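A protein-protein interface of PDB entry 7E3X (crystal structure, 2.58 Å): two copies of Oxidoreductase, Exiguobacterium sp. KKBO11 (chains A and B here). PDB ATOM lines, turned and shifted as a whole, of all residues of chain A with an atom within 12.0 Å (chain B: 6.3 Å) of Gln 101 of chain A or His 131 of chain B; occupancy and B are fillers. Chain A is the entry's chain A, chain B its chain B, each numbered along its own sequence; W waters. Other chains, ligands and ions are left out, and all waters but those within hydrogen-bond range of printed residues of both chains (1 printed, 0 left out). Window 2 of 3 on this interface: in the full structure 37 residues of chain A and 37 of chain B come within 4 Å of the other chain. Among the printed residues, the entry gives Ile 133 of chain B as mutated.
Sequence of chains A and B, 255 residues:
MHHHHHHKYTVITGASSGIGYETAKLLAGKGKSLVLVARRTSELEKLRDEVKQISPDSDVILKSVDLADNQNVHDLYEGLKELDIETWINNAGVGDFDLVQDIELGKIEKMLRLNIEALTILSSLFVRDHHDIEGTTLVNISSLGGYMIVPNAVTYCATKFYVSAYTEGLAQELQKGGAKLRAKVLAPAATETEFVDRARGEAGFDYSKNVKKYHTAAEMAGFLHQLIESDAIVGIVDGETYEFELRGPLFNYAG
The backbone NH (N) of Lys 180 of chain B is in hydrogen-bond range of the backbone carbonyl oxygen (O) of His 131 of chain B, 2.8 Å away.
The backbone carbonyl oxygen of His 131 of chain B sits at hydrogen-bond distance from the backbone NH of Leu 181 of chain B (3.1 Å).
The side-chain carboxylate (OD1) of Asp 129 of chain B is in salt-bridge range of the guanidinium group (NE) of Arg 128 of chain B (2.9 Å).
Leu 99 of chain A touches Glu 173 of chain B.
CG1 of Val 100 of chain A touches CA of Ser 124 of chain B, 3.9 Å away.
Val 100 of chain A touches Leu 170 of chain B (CG2 to CD1, 3.7 Å).
CB of Gln 101 of chain A touches CG1 of Val 127 of chain B, 3.7 Å away.
Arg 128 of chain B touches Gln 101 of chain A.
Ile 103 of chain A touches Ser 124 of chain B (CD1 to OG, 3.6 Å).
Val 154 of chain A touches Leu 170 of chain B.
Glu 173 of chain B touches Val 154 of chain A.
No position is printed for both chains.
Of the 10 pairs that touch across the chains among the printed residues, none has its exchanged pair printed and touching as well.
Water W1 lies within hydrogen-bond range of O of Asp 98 of chain A, OE1 of Glu 173 of chain B, N of Val 154 of chain A and N of Ala 153 of chain A.
Of the 19 printed residues of chain A, 5 touch a printed residue of chain B.
Of the 18 printed residues of chain B, 6 touch a printed residue of chain A.
Printed residues of chain B that touch a printed residue of chain A: Ser 124, Val 127, Arg 128, His 131, Leu 170 and Glu 173.
Along chain B the printed residues that touch a printed residue of chain A span positions 124 to 173.
Among the printed residues, no Asp or Glu carboxylate lies within 4 Å of a Lys or Arg side-chain nitrogen of the other chain.
Gln 101 of chain A touches just these residues of chain B: Val 127 (3.7 Å), Arg 128 (3.7 Å) and His 131 (3.4 Å).
Ser 124 of chain B touches two residues of chain A.
Phe 126 of chain B touches none of the printed residues of chain A.
Val 127 of chain B touches just one residue of chain A: Gln 101 (3.7 Å).
No residue of chain A comes within 4 Å of Asp 132 of chain B.
Leu 174 of chain B touches none of the printed residues of chain A.
Gly 178 of chain B touches none of the printed residues of chain A.
No residue of chain A comes within 4 Å of Ala 179 of chain B.
No residue of chain A comes within 4 Å of Leu 181 of chain B.
Printed residues of chain B within 4 Å of Val 100 of chain A: Ser 124 (3.9 Å), Leu 170 (3.7 Å) and Glu 173 (2.7 Å).
Of the printed residues of chain A, Leu 170 of chain B touches Val 100 (3.7 Å) and Val 154 (3.5 Å).
Glu 104 of chain A touches none of the printed residues of chain B.
Gly 106 of chain A touches none of the printed residues of chain B.
The nearest residue of chain B that does not touch Gln 101 of chain A is Glu 173 of chain B (4.5 Å).
The nearest printed residue of chain A that does not touch Arg 128 of chain B is Val 100 of chain A (5.5 Å).
NE2 of Gln 101 of chain A lies within hydrogen-bond range of NE2 of His 131 of chain B (3.4 Å).
OE2 of Glu 173 of chain B sits at hydrogen-bond distance from N of Val 100 of chain A (2.7 Å).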
ATOM      1  N   ASP A  96      14.636  29.631 -24.805  1.00  0.00           N
ATOM      2  CA  ASP A  96      13.261  29.758 -24.360  1.00  0.00           C
ATOM      3  C   ASP A  96      13.317  30.459 -23.019  1.00  0.00           C
ATOM      4  O   ASP A  96      14.148  30.113 -22.172  1.00  0.00           O
ATOM      5  CB  ASP A  96      12.578  28.392 -24.254  1.00  0.00           C
ATOM      6  CG  ASP A  96      11.160  28.471 -23.680  1.00  0.00           C
ATOM      7  OD1 ASP A  96      11.002  28.398 -22.435  1.00  0.00           O
ATOM      8  OD2 ASP A  96      10.207  28.585 -24.477  1.00  0.00           O
ATOM      9  N   PHE A  97      12.481  31.476 -22.860  1.00  0.00           N
ATOM     10  CA  PHE A  97      12.287  32.166 -21.593  1.00  0.00           C
ATOM     11  C   PHE A  97      10.916  31.746 -21.108  1.00  0.00           C
ATOM     12  O   PHE A  97       9.908  32.102 -21.724  1.00  0.00           O
ATOM     13  CB  PHE A  97      12.373  33.678 -21.760  1.00  0.00           C
ATOM     14  CG  PHE A  97      13.470  34.110 -22.664  1.00  0.00           C
ATOM     15  CD1 PHE A  97      14.763  33.680 -22.445  1.00  0.00           C
ATOM     16  CD2 PHE A  97      13.206  34.898 -23.765  1.00  0.00           C
ATOM     17  CE1 PHE A  97      15.781  34.066 -23.278  1.00  0.00           C
ATOM     18  CE2 PHE A  97      14.221  35.292 -24.604  1.00  0.00           C
ATOM     19  CZ  PHE A  97      15.511  34.875 -24.365  1.00  0.00           C
ATOM     20  N   ASP A  98      10.885  30.961 -20.037  1.00  0.00           N
ATOM     21  CA  ASP A  98       9.636  30.517 -19.442  1.00  0.00           C
ATOM     22  C   ASP A  98       9.906  29.621 -18.249  1.00  0.00           C
ATOM     23  O   ASP A  98      10.901  28.886 -18.232  1.00  0.00           O
ATOM     24  CB  ASP A  98       8.776  29.765 -20.446  1.00  0.00           C
ATOM     25  CG  ASP A  98       7.363  30.298 -20.495  1.00  0.00           C
ATOM     26  OD1 ASP A  98       6.892  30.829 -19.448  1.00  0.00           O
ATOM     27  OD2 ASP A  98       6.724  30.178 -21.569  1.00  0.00           O
ATOM     28  N   LEU A  99       9.033  29.688 -17.246  1.00  0.00           N
ATOM     29  CA  LEU A  99       9.090  28.736 -16.154  1.00  0.00           C
ATOM     30  C   LEU A  99       8.953  27.326 -16.714  1.00  0.00           C
ATOM     31  O   LEU A  99       8.317  27.117 -17.755  1.00  0.00           O
ATOM     32  CB  LEU A  99       7.989  29.050 -15.151  1.00  0.00           C
ATOM     33  CG  LEU A  99       8.056  30.488 -14.614  1.00  0.00           C
ATOM     34  CD1 LEU A  99       7.013  30.741 -13.536  1.00  0.00           C
ATOM     35  CD2 LEU A  99       9.448  30.784 -14.064  1.00  0.00           C
ATOM     36  N   VAL A 100       9.610  26.360 -16.051  1.00  0.00           N
ATOM     37  CA  VAL A 100       9.472  24.957 -16.457  1.00  0.00           C
ATOM     38  C   VAL A 100       8.000  24.597 -16.550  1.00  0.00           C
ATOM     39  O   VAL A 100       7.556  23.951 -17.507  1.00  0.00           O
ATOM     40  CB  VAL A 100      10.217  24.024 -15.477  1.00  0.00           C
ATOM     41  CG1 VAL A 100      10.029  22.577 -15.864  1.00  0.00           C
ATOM     42  CG2 VAL A 100      11.674  24.355 -15.423  1.00  0.00           C
ATOM     43  N   GLN A 101       7.213  25.051 -15.576  1.00  0.00           N
ATOM     44  CA  GLN A 101       5.801  24.714 -15.513  1.00  0.00           C
ATOM     45  C   GLN A 101       5.000  25.272 -16.671  1.00  0.00           C
ATOM     46  O   GLN A 101       3.831  24.911 -16.810  1.00  0.00           O
ATOM     47  CB  GLN A 101       5.203  25.230 -14.213  1.00  0.00           C
ATOM     48  CG  GLN A 101       5.173  26.733 -14.095  1.00  0.00           C
ATOM     49  CD  GLN A 101       4.836  27.158 -12.683  1.00  0.00           C
ATOM     50  OE1 GLN A 101       5.656  27.037 -11.772  1.00  0.00           O
ATOM     51  NE2 GLN A 101       3.616  27.641 -12.488  1.00  0.00           N
ATOM     52  N   ASP A 102       5.580  26.127 -17.500  1.00  0.00           N
ATOM     53  CA  ASP A 102       4.844  26.771 -18.573  1.00  0.00           C
ATOM     54  C   ASP A 102       5.351  26.417 -19.955  1.00  0.00           C
ATOM     55  O   ASP A 102       4.682  26.742 -20.946  1.00  0.00           O
ATOM     56  CB  ASP A 102       4.900  28.293 -18.413  1.00  0.00           C
ATOM     57  CG  ASP A 102       4.168  28.745 -17.224  1.00  0.00           C
ATOM     58  OD1 ASP A 102       3.159  28.086 -16.898  1.00  0.00           O
ATOM     59  OD2 ASP A 102       4.599  29.744 -16.624  1.00  0.00           O
ATOM     60  N   ILE A 103       6.515  25.776 -20.042  1.00  0.00           N
ATOM     61  CA  ILE A 103       7.113  25.492 -21.320  1.00  0.00           C
ATOM     62  C   ILE A 103       6.131  24.717 -22.162  1.00  0.00           C
ATOM     63  O   ILE A 103       5.264  23.998 -21.655  1.00  0.00           O
ATOM     64  CB  ILE A 103       8.411  24.693 -21.143  1.00  0.00           C
ATOM     65  CG1 ILE A 103       8.095  23.357 -20.471  1.00  0.00           C
ATOM     66  CG2 ILE A 103       9.433  25.494 -20.328  1.00  0.00           C
ATOM     67  CD1 ILE A 103       8.985  22.250 -20.919  1.00  0.00           C
ATOM     68  N   GLU A 104       6.260  24.875 -23.471  1.00  0.00           N
ATOM     69  CA  GLU A 104       5.626  23.969 -24.412  1.00  0.00           C
ATOM     70  C   GLU A 104       6.583  22.806 -24.634  1.00  0.00           C
ATOM     71  O   GLU A 104       7.743  23.012 -25.015  1.00  0.00           O
ATOM     72  CB  GLU A 104       5.288  24.679 -25.722  1.00  0.00           C
ATOM     73  CG  GLU A 104       4.573  26.005 -25.513  1.00  0.00           C
ATOM     74  CD  GLU A 104       4.653  26.920 -26.722  1.00  0.00           C
ATOM     75  OE1 GLU A 104       5.332  26.545 -27.706  1.00  0.00           O
ATOM     76  OE2 GLU A 104       4.044  28.017 -26.681  1.00  0.00           O
ATOM     77  N   LEU A 105       6.101  21.585 -24.381  1.00  0.00           N
ATOM     78  CA  LEU A 105       6.961  20.411 -24.494  1.00  0.00           C
ATOM     79  C   LEU A 105       7.586  20.276 -25.879  1.00  0.00           C
ATOM     80  O   LEU A 105       8.679  19.715 -26.010  1.00  0.00           O
ATOM     81  CB  LEU A 105       6.174  19.146 -24.156  1.00  0.00           C
ATOM     82  CG  LEU A 105       6.480  18.585 -22.775  1.00  0.00           C
ATOM     83  CD1 LEU A 105       7.946  18.233 -22.714  1.00  0.00           C
ATOM     84  CD2 LEU A 105       6.145  19.608 -21.711  1.00  0.00           C
ATOM     85  N   GLY A 106       6.911  20.747 -26.925  1.00  0.00           N
ATOM     86  CA  GLY A 106       7.446  20.552 -28.257  1.00  0.00           C
ATOM     87  C   GLY A 106       8.610  21.476 -28.532  1.00  0.00           C
ATOM     88  O   GLY A 106       9.614  21.076 -29.131  1.00  0.00           O
ATOM     89  N   ILE A 108      10.585  22.833 -26.250  1.00  0.00           N
ATOM     90  CA  ILE A 108      11.698  22.400 -25.422  1.00  0.00           C
ATOM     91  C   ILE A 108      12.366  21.172 -26.038  1.00  0.00           C
ATOM     92  O   ILE A 108      13.597  21.092 -26.110  1.00  0.00           O
ATOM     93  CB  ILE A 108      11.218  22.156 -23.976  1.00  0.00           C
ATOM     94  CG1 ILE A 108      11.242  23.465 -23.140  1.00  0.00           C
ATOM     95  CG2 ILE A 108      12.071  21.075 -23.300  1.00  0.00           C
ATOM     96  CD1 ILE A 108      10.693  24.730 -23.843  1.00  0.00           C
ATOM     97  N   MET A 111      14.382  22.137 -28.863  1.00  0.00           N
ATOM     98  CA  MET A 111      15.566  22.826 -28.354  1.00  0.00           C
ATOM     99  C   MET A 111      16.635  21.831 -27.925  1.00  0.00           C
ATOM    100  O   MET A 111      17.822  22.014 -28.230  1.00  0.00           O
ATOM    101  CB  MET A 111      15.199  23.754 -27.193  1.00  0.00           C
ATOM    102  CG  MET A 111      16.368  24.592 -26.662  1.00  0.00           C
ATOM    103  SD  MET A 111      15.927  25.785 -25.369  1.00  0.00           S
ATOM    104  CE  MET A 111      15.233  24.748 -24.077  1.00  0.00           C
ATOM    105  N   PRO A 151      17.752  32.761 -14.176  1.00  0.00           N
ATOM    106  CA  PRO A 151      16.327  32.554 -13.901  1.00  0.00           C
ATOM    107  C   PRO A 151      15.490  32.728 -15.161  1.00  0.00           C
ATOM    108  O   PRO A 151      15.844  33.479 -16.069  1.00  0.00           O
ATOM    109  CB  PRO A 151      16.002  33.626 -12.853  1.00  0.00           C
ATOM    110  CG  PRO A 151      17.292  33.939 -12.226  1.00  0.00           C
ATOM    111  CD  PRO A 151      18.330  33.805 -13.314  1.00  0.00           C
ATOM    112  N   ASN A 152      14.389  31.991 -15.218  1.00  0.00           N
ATOM    113  CA  ASN A 152      13.431  32.007 -16.309  1.00  0.00           C
ATOM    114  C   ASN A 152      14.001  31.458 -17.607  1.00  0.00           C
ATOM    115  O   ASN A 152      13.368  31.587 -18.666  1.00  0.00           O
ATOM    116  CB  ASN A 152      12.855  33.403 -16.546  1.00  0.00           C
ATOM    117  CG  ASN A 152      11.380  33.348 -16.897  1.00  0.00           C
ATOM    118  OD1 ASN A 152      10.521  33.305 -16.014  1.00  0.00           O
ATOM    119  ND2 ASN A 152      11.080  33.292 -18.195  1.00  0.00           N
ATOM    120  N   ALA A 153      15.146  30.794 -17.552  1.00  0.00           N
ATOM    121  CA  ALA A 153      15.708  30.151 -18.729  1.00  0.00           C
ATOM    122  C   ALA A 153      16.417  28.867 -18.300  1.00  0.00           C
ATOM    123  O   ALA A 153      17.549  28.585 -18.700  1.00  0.00           O
ATOM    124  CB  ALA A 153      16.646  31.109 -19.461  1.00  0.00           C
ATOM    125  N   VAL A 154      15.748  28.072 -17.463  1.00  0.00           N
ATOM    126  CA  VAL A 154      16.434  26.961 -16.809  1.00  0.00           C
ATOM    127  C   VAL A 154      16.828  25.900 -17.828  1.00  0.00           C
ATOM    128  O   VAL A 154      17.994  25.500 -17.903  1.00  0.00           O
ATOM    129  CB  VAL A 154      15.561  26.384 -15.682  1.00  0.00           C
ATOM    130  CG1 VAL A 154      16.063  25.020 -15.238  1.00  0.00           C
ATOM    131  CG2 VAL A 154      15.533  27.332 -14.527  1.00  0.00           C
ATOM    132  N   THR A 155      15.873  25.463 -18.660  1.00  0.00           N
ATOM    133  CA  THR A 155      16.155  24.395 -19.615  1.00  0.00           C
ATOM    134  C   THR A 155      17.229  24.797 -20.623  1.00  0.00           C
ATOM    135  O   THR A 155      18.101  23.984 -20.961  1.00  0.00           O
ATOM    136  CB  THR A 155      14.880  23.991 -20.355  1.00  0.00           C
ATOM    137  OG1 THR A 155      13.815  23.858 -19.417  1.00  0.00           O
ATOM    138  CG2 THR A 155      15.089  22.670 -21.096  1.00  0.00           C
ATOM    139  N   TYR A 156      17.152  26.024 -21.156  1.00  0.00           N
ATOM    140  CA  TYR A 156      18.141  26.469 -22.134  1.00  0.00           C
ATOM    141  C   TYR A 156      19.535  26.467 -21.520  1.00  0.00           C
ATOM    142  O   TYR A 156      20.475  25.877 -22.075  1.00  0.00           O
ATOM    143  CB  TYR A 156      17.780  27.859 -22.654  1.00  0.00           C
ATOM    144  CG  TYR A 156      18.910  28.562 -23.383  1.00  0.00           C
ATOM    145  CD1 TYR A 156      19.242  28.223 -24.685  1.00  0.00           C
ATOM    146  CD2 TYR A 156      19.636  29.572 -22.768  1.00  0.00           C
ATOM    147  CE1 TYR A 156      20.266  28.873 -25.355  1.00  0.00           C
ATOM    148  CE2 TYR A 156      20.663  30.228 -23.436  1.00  0.00           C
ATOM    149  CZ  TYR A 156      20.977  29.871 -24.724  1.00  0.00           C
ATOM    150  OH  TYR A 156      22.002  30.522 -25.388  1.00  0.00           O
ATOM    151  N   SER B 124       9.254  18.116 -16.509  1.00  0.00           N
ATOM    152  CA  SER B 124       8.406  19.234 -16.920  1.00  0.00           C
ATOM    153  C   SER B 124       6.940  18.924 -16.698  1.00  0.00           C
ATOM    154  O   SER B 124       6.185  19.774 -16.200  1.00  0.00           O
ATOM    155  CB  SER B 124       8.657  19.583 -18.395  1.00  0.00           C
ATOM    156  OG  SER B 124      10.030  19.539 -18.730  1.00  0.00           O
ATOM    157  N   PHE B 126       5.663  16.711 -14.689  1.00  0.00           N
ATOM    158  CA  PHE B 126       5.397  16.596 -13.265  1.00  0.00           C
ATOM    159  C   PHE B 126       5.325  17.977 -12.608  1.00  0.00           C
ATOM    160  O   PHE B 126       4.422  18.245 -11.803  1.00  0.00           O
ATOM    161  CB  PHE B 126       6.467  15.718 -12.611  1.00  0.00           C
ATOM    162  CG  PHE B 126       6.168  15.370 -11.187  1.00  0.00           C
ATOM    163  CD1 PHE B 126       5.091  14.561 -10.876  1.00  0.00           C
ATOM    164  CD2 PHE B 126       6.947  15.850 -10.161  1.00  0.00           C
ATOM    165  CE1 PHE B 126       4.801  14.245  -9.561  1.00  0.00           C
ATOM    166  CE2 PHE B 126       6.667  15.524  -8.854  1.00  0.00           C
ATOM    167  CZ  PHE B 126       5.587  14.721  -8.554  1.00  0.00           C
ATOM    168  N   VAL B 127       6.261  18.867 -12.965  1.00  0.00           N
ATOM    169  CA  VAL B 127       6.270  20.241 -12.461  1.00  0.00           C
ATOM    170  C   VAL B 127       4.976  20.960 -12.827  1.00  0.00           C
ATOM    171  O   VAL B 127       4.345  21.613 -11.987  1.00  0.00           O
ATOM    172  CB  VAL B 127       7.497  20.994 -13.007  1.00  0.00           C
ATOM    173  CG1 VAL B 127       7.308  22.496 -12.863  1.00  0.00           C
ATOM    174  CG2 VAL B 127       8.731  20.578 -12.267  1.00  0.00           C
ATOM    175  N   ARG B 128       4.586  20.868 -14.096  1.00  0.00           N
ATOM    176  CA  ARG B 128       3.324  21.421 -14.567  1.00  0.00           C
ATOM    177  C   ARG B 128       2.171  21.053 -13.640  1.00  0.00           C
ATOM    178  O   ARG B 128       1.427  21.925 -13.174  1.00  0.00           O
ATOM    179  CB  ARG B 128       3.057  20.917 -15.985  1.00  0.00           C
ATOM    180  CG  ARG B 128       1.952  21.685 -16.692  1.00  0.00           C
ATOM    181  CD  ARG B 128       1.469  20.954 -17.930  1.00  0.00           C
ATOM    182  NE  ARG B 128       1.007  19.605 -17.605  1.00  0.00           N
ATOM    183  CZ  ARG B 128       0.761  18.658 -18.505  1.00  0.00           C
ATOM    184  NH1 ARG B 128       0.924  18.907 -19.805  1.00  0.00           N
ATOM    185  NH2 ARG B 128       0.365  17.459 -18.100  1.00  0.00           N
ATOM    186  N   ASP B 129       2.046  19.766 -13.318  1.00  0.00           N
ATOM    187  CA  ASP B 129       0.891  19.249 -12.611  1.00  0.00           C
ATOM    188  C   ASP B 129       1.027  19.264 -11.092  1.00  0.00           C
ATOM    189  O   ASP B 129       0.003  19.230 -10.398  1.00  0.00           O
ATOM    190  CB  ASP B 129       0.602  17.823 -13.081  1.00  0.00           C
ATOM    191  CG  ASP B 129       0.202  17.762 -14.550  1.00  0.00           C
ATOM    192  OD1 ASP B 129      -0.293  18.780 -15.092  1.00  0.00           O
ATOM    193  OD2 ASP B 129       0.383  16.694 -15.169  1.00  0.00           O
ATOM    194  N   HIS B 130       2.239  19.338 -10.546  1.00  0.00           N
ATOM    195  CA  HIS B 130       2.389  19.240  -9.099  1.00  0.00           C
ATOM    196  C   HIS B 130       3.058  20.447  -8.459  1.00  0.00           C
ATOM    197  O   HIS B 130       3.407  20.374  -7.273  1.00  0.00           O
ATOM    198  CB  HIS B 130       3.157  17.968  -8.741  1.00  0.00           C
ATOM    199  CG  HIS B 130       2.540  16.729  -9.301  1.00  0.00           C
ATOM    200  ND1 HIS B 130       2.668  16.370 -10.626  1.00  0.00           N
ATOM    201  CD2 HIS B 130       1.760  15.786  -8.726  1.00  0.00           C
ATOM    202  CE1 HIS B 130       2.000  15.251 -10.839  1.00  0.00           C
ATOM    203  NE2 HIS B 130       1.447  14.872  -9.700  1.00  0.00           N
ATOM    204  N   HIS B 131       3.201  21.574  -9.175  1.00  0.00           N
ATOM    205  CA  HIS B 131       4.003  22.663  -8.612  1.00  0.00           C
ATOM    206  C   HIS B 131       3.343  23.301  -7.393  1.00  0.00           C
ATOM    207  O   HIS B 131       4.047  23.745  -6.480  1.00  0.00           O
ATOM    208  CB  HIS B 131       4.320  23.718  -9.673  1.00  0.00           C
ATOM    209  CG  HIS B 131       3.128  24.470 -10.170  1.00  0.00           C
ATOM    210  ND1 HIS B 131       2.599  25.552  -9.499  1.00  0.00           N
ATOM    211  CD2 HIS B 131       2.384  24.322 -11.294  1.00  0.00           C
ATOM    212  CE1 HIS B 131       1.575  26.032 -10.184  1.00  0.00           C
ATOM    213  NE2 HIS B 131       1.422  25.303 -11.275  1.00  0.00           N
ATOM    214  N   ASP B 132       2.010  23.324  -7.331  1.00  0.00           N
ATOM    215  CA  ASP B 132       1.308  23.866  -6.169  1.00  0.00           C
ATOM    216  C   ASP B 132       0.629  22.788  -5.316  1.00  0.00           C
ATOM    217  O   ASP B 132      -0.247  23.110  -4.510  1.00  0.00           O
ATOM    218  CB  ASP B 132       0.288  24.934  -6.586  1.00  0.00           C
ATOM    219  CG  ASP B 132      -0.724  24.423  -7.592  1.00  0.00           C
ATOM    220  OD1 ASP B 132      -0.418  23.475  -8.345  1.00  0.00           O
ATOM    221  OD2 ASP B 132      -1.838  24.980  -7.639  1.00  0.00           O
ATOM    222  N   ILE B 133       1.032  21.527  -5.452  1.00  0.00           N
ATOM    223  CA  ILE B 133       0.473  20.435  -4.660  1.00  0.00           C
ATOM    224  C   ILE B 133       1.410  20.155  -3.488  1.00  0.00           C
ATOM    225  O   ILE B 133       2.559  19.736  -3.681  1.00  0.00           O
ATOM    226  CB  ILE B 133       0.261  19.164  -5.505  1.00  0.00           C
ATOM    227  CG1 ILE B 133      -1.000  19.270  -6.368  1.00  0.00           C
ATOM    228  CG2 ILE B 133       0.126  17.937  -4.593  1.00  0.00           C
ATOM    229  CD1 ILE B 133      -0.923  20.246  -7.484  1.00  0.00           C
ATOM    230  N   GLU B 134       0.918  20.358  -2.267  1.00  0.00           N
ATOM    231  CA  GLU B 134       1.754  20.181  -1.084  1.00  0.00           C
ATOM    232  C   GLU B 134       2.315  18.761  -1.014  1.00  0.00           C
ATOM    233  O   GLU B 134       1.670  17.799  -1.438  1.00  0.00           O
ATOM    234  CB  GLU B 134       0.937  20.497   0.177  1.00  0.00           C
ATOM    235  CG  GLU B 134       1.628  21.474   1.098  1.00  0.00           C
ATOM    236  CD  GLU B 134       2.806  20.841   1.823  1.00  0.00           C
ATOM    237  OE1 GLU B 134       2.634  19.706   2.320  1.00  0.00           O
ATOM    238  OE2 GLU B 134       3.908  21.454   1.849  1.00  0.00           O
ATOM    239  N   THR B 136       4.797  17.186  -2.602  1.00  0.00           N
ATOM    240  CA  THR B 136       5.360  16.502  -3.762  1.00  0.00           C
ATOM    241  C   THR B 136       6.848  16.775  -3.876  1.00  0.00           C
ATOM    242  O   THR B 136       7.299  17.890  -3.604  1.00  0.00           O
ATOM    243  CB  THR B 136       4.671  16.947  -5.048  1.00  0.00           C
ATOM    244  OG1 THR B 136       4.767  18.373  -5.157  1.00  0.00           O
ATOM    245  CG2 THR B 136       3.219  16.538  -5.023  1.00  0.00           C
ATOM    246  N   LEU B 170      15.850  24.424 -11.758  1.00  0.00           N
ATOM    247  CA  LEU B 170      14.448  24.134 -11.467  1.00  0.00           C
ATOM    248  C   LEU B 170      14.156  24.221  -9.969  1.00  0.00           C
ATOM    249  O   LEU B 170      13.151  24.816  -9.553  1.00  0.00           O
ATOM    250  CB  LEU B 170      14.104  22.751 -12.011  1.00  0.00           C
ATOM    251  CG  LEU B 170      12.781  22.137 -11.562  1.00  0.00           C
ATOM    252  CD1 LEU B 170      11.630  23.070 -11.908  1.00  0.00           C
ATOM    253  CD2 LEU B 170      12.590  20.738 -12.173  1.00  0.00           C
ATOM    254  N   GLU B 173      14.163  27.833  -9.139  1.00  0.00           N
ATOM    255  CA  GLU B 173      12.954  28.406  -9.721  1.00  0.00           C
ATOM    256  C   GLU B 173      11.743  28.176  -8.827  1.00  0.00           C
ATOM    257  O   GLU B 173      10.955  29.098  -8.581  1.00  0.00           O
ATOM    258  CB  GLU B 173      12.704  27.795 -11.095  1.00  0.00           C
ATOM    259  CG  GLU B 173      11.462  28.302 -11.810  1.00  0.00           C
ATOM    260  CD  GLU B 173      11.528  28.007 -13.299  1.00  0.00           C
ATOM    261  OE1 GLU B 173      12.404  28.603 -13.973  1.00  0.00           O
ATOM    262  OE2 GLU B 173      10.738  27.164 -13.790  1.00  0.00           O
ATOM    263  N   LEU B 174      11.566  26.947  -8.337  1.00  0.00           N
ATOM    264  CA  LEU B 174      10.380  26.658  -7.542  1.00  0.00           C
ATOM    265  C   LEU B 174      10.421  27.403  -6.218  1.00  0.00           C
ATOM    266  O   LEU B 174       9.384  27.866  -5.726  1.00  0.00           O
ATOM    267  CB  LEU B 174      10.247  25.155  -7.317  1.00  0.00           C
ATOM    268  CG  LEU B 174      10.160  24.311  -8.593  1.00  0.00           C
ATOM    269  CD1 LEU B 174      10.495  22.857  -8.288  1.00  0.00           C
ATOM    270  CD2 LEU B 174       8.796  24.420  -9.262  1.00  0.00           C
ATOM    271  N   GLY B 178       7.727  30.213  -4.703  1.00  0.00           N
ATOM    272  CA  GLY B 178       6.901  29.733  -3.609  1.00  0.00           C
ATOM    273  C   GLY B 178       6.166  28.449  -3.907  1.00  0.00           C
ATOM    274  O   GLY B 178       5.146  28.169  -3.268  1.00  0.00           O
ATOM    275  N   ALA B 179       6.645  27.660  -4.870  1.00  0.00           N
ATOM    276  CA  ALA B 179       5.969  26.419  -5.206  1.00  0.00           C
ATOM    277  C   ALA B 179       5.953  25.486  -3.995  1.00  0.00           C
ATOM    278  O   ALA B 179       6.825  25.549  -3.130  1.00  0.00           O
ATOM    279  CB  ALA B 179       6.659  25.743  -6.391  1.00  0.00           C
ATOM    280  N   LYS B 180       4.929  24.632  -3.922  1.00  0.00           N
ATOM    281  CA  LYS B 180       4.918  23.603  -2.889  1.00  0.00           C
ATOM    282  C   LYS B 180       5.822  22.435  -3.262  1.00  0.00           C
ATOM    283  O   LYS B 180       6.515  21.879  -2.404  1.00  0.00           O
ATOM    284  CB  LYS B 180       3.489  23.119  -2.642  1.00  0.00           C
ATOM    285  CG  LYS B 180       2.609  24.130  -1.925  1.00  0.00           C
ATOM    286  CD  LYS B 180       3.155  24.452  -0.528  1.00  0.00           C
ATOM    287  CE  LYS B 180       2.093  25.122   0.361  1.00  0.00           C
ATOM    288  NZ  LYS B 180       1.795  26.518  -0.046  1.00  0.00           N
ATOM    289  N   LEU B 181       5.833  22.059  -4.537  1.00  0.00           N
ATOM    290  CA  LEU B 181       6.733  21.017  -5.024  1.00  0.00           C
ATOM    291  C   LEU B 181       8.191  21.343  -4.706  1.00  0.00           C
ATOM    292  O   LEU B 181       8.619  22.498  -4.791  1.00  0.00           O
ATOM    293  CB  LEU B 181       6.550  20.852  -6.531  1.00  0.00           C
ATOM    294  CG  LEU B 181       7.633  20.090  -7.292  1.00  0.00           C
ATOM    295  CD1 LEU B 181       7.607  18.636  -6.915  1.00  0.00           C
ATOM    296  CD2 LEU B 181       7.413  20.266  -8.783  1.00  0.00           C
HETATM  297  O   HOH W   1      12.925  28.280 -16.748  1.00  0.00           O
